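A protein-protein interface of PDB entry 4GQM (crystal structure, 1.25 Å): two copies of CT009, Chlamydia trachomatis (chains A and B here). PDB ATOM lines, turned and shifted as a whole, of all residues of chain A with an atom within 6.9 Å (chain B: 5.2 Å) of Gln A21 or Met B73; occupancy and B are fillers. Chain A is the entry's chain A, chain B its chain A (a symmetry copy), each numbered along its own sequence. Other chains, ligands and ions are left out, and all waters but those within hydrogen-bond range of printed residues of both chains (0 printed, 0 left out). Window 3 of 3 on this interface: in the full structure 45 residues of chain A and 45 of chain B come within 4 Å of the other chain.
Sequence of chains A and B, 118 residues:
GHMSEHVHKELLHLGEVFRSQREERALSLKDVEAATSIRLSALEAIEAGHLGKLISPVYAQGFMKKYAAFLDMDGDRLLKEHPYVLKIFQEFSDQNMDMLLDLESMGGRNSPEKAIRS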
ATOM      1  N   LEU A  14      14.342   4.611  14.964  1.00  0.00           N
ATOM      2  CA  LEU A  14      15.481   4.148  14.228  1.00  0.00           C
ATOM      3  C   LEU A  14      15.513   2.615  14.211  1.00  0.00           C
ATOM      4  O   LEU A  14      15.768   1.980  13.180  1.00  0.00           O
ATOM      5  CB  LEU A  14      16.735   4.735  14.883  1.00  0.00           C
ATOM      6  CG  LEU A  14      18.058   4.376  14.279  1.00  0.00           C
ATOM      7  CD1 LEU A  14      18.083   4.740  12.804  1.00  0.00           C
ATOM      8  CD2 LEU A  14      19.108   5.115  15.045  1.00  0.00           C
ATOM      9  N   GLU A  16      13.068   0.598  14.434  1.00  0.00           N
ATOM     10  CA  GLU A  16      12.018   0.136  13.550  1.00  0.00           C
ATOM     11  C   GLU A  16      12.367   0.311  12.078  1.00  0.00           C
ATOM     12  O   GLU A  16      11.954  -0.492  11.265  1.00  0.00           O
ATOM     13  CB  GLU A  16      10.729   0.872  13.901  1.00  0.00           C
ATOM     14  CG  GLU A  16      10.070   0.329  15.166  1.00  0.00           C
ATOM     15  CD  GLU A  16       9.673  -1.141  15.031  1.00  0.00           C
ATOM     16  OE1 GLU A  16       9.129  -1.497  13.963  1.00  0.00           O
ATOM     17  OE2 GLU A  16       9.902  -1.925  15.983  1.00  0.00           O
ATOM     18  N   VAL A  17      13.145   1.333  11.747  1.00  0.00           N
ATOM     19  CA  VAL A  17      13.627   1.483  10.359  1.00  0.00           C
ATOM     20  C   VAL A  17      14.488   0.251  10.001  1.00  0.00           C
ATOM     21  O   VAL A  17      14.328  -0.375   8.956  1.00  0.00           O
ATOM     22  CB  VAL A  17      14.436   2.775  10.155  1.00  0.00           C
ATOM     23  CG1 VAL A  17      15.098   2.773   8.785  1.00  0.00           C
ATOM     24  CG2 VAL A  17      13.543   4.002  10.289  1.00  0.00           C
ATOM     25  N   PHE A  18      15.436  -0.089  10.880  1.00  0.00           N
ATOM     26  CA  PHE A  18      16.281  -1.263  10.661  1.00  0.00           C
ATOM     27  C   PHE A  18      15.442  -2.531  10.553  1.00  0.00           C
ATOM     28  O   PHE A  18      15.592  -3.303   9.610  1.00  0.00           O
ATOM     29  CB  PHE A  18      17.329  -1.403  11.775  1.00  0.00           C
ATOM     30  CG  PHE A  18      18.472  -0.456  11.660  1.00  0.00           C
ATOM     31  CD1 PHE A  18      19.483  -0.693  10.752  1.00  0.00           C
ATOM     32  CD2 PHE A  18      18.629   0.600  12.521  1.00  0.00           C
ATOM     33  CE1 PHE A  18      20.564   0.146  10.685  1.00  0.00           C
ATOM     34  CE2 PHE A  18      19.749   1.453  12.428  1.00  0.00           C
ATOM     35  CZ  PHE A  18      20.682   1.229  11.507  1.00  0.00           C
ATOM     36  N   ARG A  19      14.550  -2.741  11.509  1.00  0.00           N
ATOM     37  CA  ARG A  19      13.757  -3.962  11.522  1.00  0.00           C
ATOM     38  C   ARG A  19      12.906  -4.064  10.259  1.00  0.00           C
ATOM     39  O   ARG A  19      12.813  -5.129   9.640  1.00  0.00           O
ATOM     40  CB  ARG A  19      12.876  -4.016  12.758  1.00  0.00           C
ATOM     41  CG  ARG A  19      12.027  -5.276  12.900  1.00  0.00           C
ATOM     42  CD  ARG A  19      10.957  -5.026  14.038  1.00  0.00           C
ATOM     43  NE  ARG A  19      11.386  -5.339  15.390  1.00  0.00           N
ATOM     44  CZ  ARG A  19      11.822  -4.494  16.339  1.00  0.00           C
ATOM     45  NH1 ARG A  19      11.968  -3.172  16.154  1.00  0.00           N
ATOM     46  NH2 ARG A  19      12.124  -5.013  17.524  1.00  0.00           N
ATOM     47  N   SER A  20      12.266  -2.977   9.843  1.00  0.00           N
ATOM     48  CA  SER A  20      11.428  -2.975   8.649  1.00  0.00           C
ATOM     49  C   SER A  20      12.213  -3.377   7.423  1.00  0.00           C
ATOM     50  O   SER A  20      11.749  -4.168   6.588  1.00  0.00           O
ATOM     51  CB  SER A  20      10.845  -1.590   8.416  1.00  0.00           C
ATOM     52  OG  SER A  20       9.887  -1.286   9.408  1.00  0.00           O
ATOM     53  N   GLN A  21      13.407  -2.816   7.277  1.00  0.00           N
ATOM     54  CA  GLN A  21      14.236  -3.115   6.118  1.00  0.00           C
ATOM     55  C   GLN A  21      14.733  -4.555   6.126  1.00  0.00           C
ATOM     56  O   GLN A  21      14.759  -5.227   5.095  1.00  0.00           O
ATOM     57  CB  GLN A  21      15.395  -2.121   6.008  1.00  0.00           C
ATOM     58  CG  GLN A  21      14.947  -0.703   5.674  1.00  0.00           C
ATOM     59  CD  GLN A  21      14.242  -0.648   4.351  1.00  0.00           C
ATOM     60  OE1 GLN A  21      14.837  -0.994   3.337  1.00  0.00           O
ATOM     61  NE2 GLN A  21      12.974  -0.220   4.343  1.00  0.00           N
ATOM     62  N   ARG A  22      15.106  -5.043   7.300  1.00  0.00           N
ATOM     63  CA  ARG A  22      15.481  -6.443   7.437  1.00  0.00           C
ATOM     64  C   ARG A  22      14.335  -7.387   7.071  1.00  0.00           C
ATOM     65  O   ARG A  22      14.514  -8.376   6.351  1.00  0.00           O
ATOM     66  CB  ARG A  22      15.967  -6.714   8.878  1.00  0.00           C
ATOM     67  CG  ARG A  22      16.360  -8.158   9.095  1.00  0.00           C
ATOM     68  CD  ARG A  22      16.820  -8.467  10.484  1.00  0.00           C
ATOM     69  NE  ARG A  22      15.889  -8.090  11.539  1.00  0.00           N
ATOM     70  CZ  ARG A  22      14.865  -8.830  11.943  1.00  0.00           C
ATOM     71  NH1 ARG A  22      14.557  -9.982  11.339  1.00  0.00           N
ATOM     72  NH2 ARG A  22      14.135  -8.406  12.967  1.00  0.00           N
ATOM     73  N   GLU A  23      13.151  -7.091   7.605  1.00  0.00           N
ATOM     74  CA  GLU A  23      11.988  -7.925   7.359  1.00  0.00           C
ATOM     75  C   GLU A  23      11.561  -7.874   5.897  1.00  0.00           C
ATOM     76  O   GLU A  23      11.088  -8.881   5.353  1.00  0.00           O
ATOM     77  CB  GLU A  23      10.847  -7.521   8.287  1.00  0.00           C
ATOM     78  CG  GLU A  23      11.088  -7.948   9.729  1.00  0.00           C
ATOM     79  CD  GLU A  23       9.963  -7.548  10.665  1.00  0.00           C
ATOM     80  OE1 GLU A  23       9.095  -6.759  10.240  1.00  0.00           O
ATOM     81  OE2 GLU A  23      10.002  -7.950  11.835  1.00  0.00           O
ATOM     82  N   GLU A  24      11.764  -6.745   5.218  1.00  0.00           N
ATOM     83  CA  GLU A  24      11.460  -6.668   3.784  1.00  0.00           C
ATOM     84  C   GLU A  24      12.256  -7.691   3.009  1.00  0.00           C
ATOM     85  O   GLU A  24      11.760  -8.307   2.062  1.00  0.00           O
ATOM     86  CB  GLU A  24      11.752  -5.254   3.301  1.00  0.00           C
ATOM     87  CG  GLU A  24      11.682  -5.093   1.807  1.00  0.00           C
ATOM     88  CD  GLU A  24      11.739  -3.634   1.343  1.00  0.00           C
ATOM     89  OE1 GLU A  24      11.284  -2.733   2.076  1.00  0.00           O
ATOM     90  OE2 GLU A  24      12.239  -3.416   0.228  1.00  0.00           O
ATOM     91  N   ARG A  25      13.496  -7.901   3.439  1.00  0.00           N
ATOM     92  CA  ARG A  25      14.396  -8.855   2.796  1.00  0.00           C
ATOM     93  C   ARG A  25      14.220 -10.288   3.319  1.00  0.00           C
ATOM     94  O   ARG A  25      14.890 -11.206   2.864  1.00  0.00           O
ATOM     95  CB  ARG A  25      15.856  -8.402   3.035  1.00  0.00           C
ATOM     96  CG  ARG A  25      16.218  -7.090   2.350  1.00  0.00           C
ATOM     97  CD  ARG A  25      17.743  -6.794   2.516  1.00  0.00           C
ATOM     98  NE  ARG A  25      18.581  -7.825   1.848  1.00  0.00           N
ATOM     99  CZ  ARG A  25      19.915  -7.836   1.868  1.00  0.00           C
ATOM    100  NH1 ARG A  25      20.555  -6.885   2.546  1.00  0.00           N
ATOM    101  NH2 ARG A  25      20.625  -8.790   1.253  1.00  0.00           N
ATOM    102  N   ALA A  26      13.335 -10.452   4.276  1.00  0.00           N
ATOM    103  CA  ALA A  26      13.037 -11.734   4.902  1.00  0.00           C
ATOM    104  C   ALA A  26      14.283 -12.392   5.511  1.00  0.00           C
ATOM    105  O   ALA A  26      14.482 -13.603   5.422  1.00  0.00           O
ATOM    106  CB  ALA A  26      12.316 -12.672   3.926  1.00  0.00           C
ATOM    107  N   LEU A  27      15.106 -11.584   6.154  1.00  0.00           N
ATOM    108  CA  LEU A  27      16.293 -12.058   6.842  1.00  0.00           C
ATOM    109  C   LEU A  27      16.044 -12.083   8.331  1.00  0.00           C
ATOM    110  O   LEU A  27      15.355 -11.210   8.864  1.00  0.00           O
ATOM    111  CB  LEU A  27      17.438 -11.113   6.541  1.00  0.00           C
ATOM    112  CG  LEU A  27      17.849 -11.013   5.080  1.00  0.00           C
ATOM    113  CD1 LEU A  27      18.945  -9.941   4.921  1.00  0.00           C
ATOM    114  CD2 LEU A  27      18.284 -12.388   4.548  1.00  0.00           C
ATOM    115  N   ALA B  68      23.333  -0.499   8.529  1.00  0.00           N
ATOM    116  CA  ALA B  68      22.666   0.271   7.486  1.00  0.00           C
ATOM    117  C   ALA B  68      23.264  -0.060   6.133  1.00  0.00           C
ATOM    118  O   ALA B  68      22.524  -0.230   5.152  1.00  0.00           O
ATOM    119  CB  ALA B  68      22.775   1.730   7.778  1.00  0.00           C
ATOM    120  N   ALA B  69      24.587  -0.110   6.036  1.00  0.00           N
ATOM    121  CA  ALA B  69      25.206  -0.419   4.748  1.00  0.00           C
ATOM    122  C   ALA B  69      24.803  -1.793   4.239  1.00  0.00           C
ATOM    123  O   ALA B  69      24.536  -1.962   3.052  1.00  0.00           O
ATOM    124  CB  ALA B  69      26.690  -0.292   4.856  1.00  0.00           C
ATOM    125  N   LEU B  71      22.060  -3.214   4.693  1.00  0.00           N
ATOM    126  CA  LEU B  71      20.681  -3.077   4.234  1.00  0.00           C
ATOM    127  C   LEU B  71      20.531  -2.054   3.111  1.00  0.00           C
ATOM    128  O   LEU B  71      19.412  -1.647   2.795  1.00  0.00           O
ATOM    129  CB  LEU B  71      19.793  -2.688   5.410  1.00  0.00           C
ATOM    130  CG  LEU B  71      19.636  -3.727   6.526  1.00  0.00           C
ATOM    131  CD1 LEU B  71      18.841  -3.111   7.672  1.00  0.00           C
ATOM    132  CD2 LEU B  71      18.992  -5.017   6.038  1.00  0.00           C
ATOM    133  N   ASP B  72      21.641  -1.621   2.506  1.00  0.00           N
ATOM    134  CA  ASP B  72      21.588  -0.680   1.364  1.00  0.00           C
ATOM    135  C   ASP B  72      20.959   0.652   1.739  1.00  0.00           C
ATOM    136  O   ASP B  72      20.347   1.313   0.899  1.00  0.00           O
ATOM    137  CB  ASP B  72      20.912  -1.323   0.141  1.00  0.00           C
ATOM    138  CG  ASP B  72      21.637  -2.576  -0.268  1.00  0.00           C
ATOM    139  OD1 ASP B  72      22.843  -2.468  -0.540  1.00  0.00           O
ATOM    140  OD2 ASP B  72      21.041  -3.663  -0.226  1.00  0.00           O
ATOM    141  N   MET B  73      21.139   1.058   2.984  1.00  0.00           N
ATOM    142  CA  MET B  73      20.739   2.383   3.435  1.00  0.00           C
ATOM    143  C   MET B  73      21.966   3.257   3.627  1.00  0.00           C
ATOM    144  O   MET B  73      23.051   2.762   3.963  1.00  0.00           O
ATOM    145  CB  MET B  73      19.969   2.304   4.744  1.00  0.00           C
ATOM    146  CG  MET B  73      18.620   1.606   4.618  1.00  0.00           C
ATOM    147  SD  MET B  73      17.588   1.765   6.081  1.00  0.00           S
ATOM    148  CE  MET B  73      18.458   0.616   7.114  1.00  0.00           C
ATOM    149  N   ASP B  74      21.779   4.561   3.469  1.00  0.00           N
ATOM    150  CA  ASP B  74      22.805   5.545   3.749  1.00  0.00           C
ATOM    151  C   ASP B  74      22.779   5.817   5.255  1.00  0.00           C
ATOM    152  O   ASP B  74      21.934   6.549   5.756  1.00  0.00           O
ATOM    153  CB  ASP B  74      22.499   6.816   2.968  1.00  0.00           C
ATOM    154  CG  ASP B  74      23.533   7.897   3.166  1.00  0.00           C
ATOM    155  OD1 ASP B  74      24.339   7.831   4.118  1.00  0.00           O
ATOM    156  OD2 ASP B  74      23.530   8.815   2.322  1.00  0.00           O
ATOM    157  N   GLY B  75      23.694   5.202   5.986  1.00  0.00           N
ATOM    158  CA  GLY B  75      23.733   5.321   7.432  1.00  0.00           C
ATOM    159  C   GLY B  75      24.007   6.735   7.898  1.00  0.00           C
ATOM    160  O   GLY B  75      23.506   7.145   8.936  1.00  0.00           O
ATOM    161  N   LEU B  78      20.728   8.469   7.553  1.00  0.00           N
ATOM    162  CA  LEU B  78      19.792   7.926   8.519  1.00  0.00           C
ATOM    163  C   LEU B  78      20.056   8.526   9.909  1.00  0.00           C
ATOM    164  O   LEU B  78      19.113   8.941  10.617  1.00  0.00           O
ATOM    165  CB  LEU B  78      19.874   6.391   8.505  1.00  0.00           C
ATOM    166  CG  LEU B  78      18.987   5.648   9.487  1.00  0.00           C
ATOM    167  CD1 LEU B  78      17.535   5.961   9.230  1.00  0.00           C
ATOM    168  CD2 LEU B  78      19.237   4.159   9.389  1.00  0.00           C
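The backbone carbonyl oxygen (O) of Ala B68 is in hydrogen-bond range of the backbone NH (N) of Met B73, at 2.9 Å.
CG of Leu B78 touches CD1 of Leu A14 (3.6 Å). SD of Met B73 touches CG1 of Val A17, at 3.8 Å. N of Ala B68 touches CE1 of Phe A18, at 3.6 Å. CD1 of Leu B71 touches O of Phe A18, at 3.8 Å. CD1 of Phe A18 touches CE of Met B73, 3.9999 Å away. Phe A18 touches Leu B78. CD1 of Leu B71 touches CB of Gln A21, at 3.95 Å. Met B73 touches Gln A21 (SD to CG, 3.6 Å).
Of the printed residues of chain B, Val A17 touches Met B73 (3.8 Å). Of the printed residues of chain B, Gln A21 touches Leu B71 (3.95 Å) and Met B73 (3.6 Å). Printed residues of chain A within 4 Å of Ala B68: Phe A18 (3.6 Å). Of the printed residues of chain A, Met B73 touches Val A17, Phe A18 and Gln A21. Of the printed residues of chain A, Leu B78 touches Leu A14 and Phe A18. The nearest printed residue of chain B that does not touch Gln A21 is Asp B72 (6.5 Å). The nearest printed residue of chain A that does not touch Met B73 is Arg A22 (6.6 Å).
Printed residues of chain B that touch a printed residue of chain A: Ala B68, Leu B71, Met B73 and Leu B78. Of the 13 printed residues of chain A, 4 touch a printed residue of chain B. Hydrophobic or aromatic side chains of chain A that line the printed part of chain B: Leu A14, Val A17 and Phe A18. Among the printed residues, no Asp or Glu carboxylate lies within 4 Å of a Lys or Arg side-chain nitrogen of the other chain.
No position is printed for both chains. Of the 8 pairs that touch across the chains among the printed residues, none has its exchanged pair printed and touching as well.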
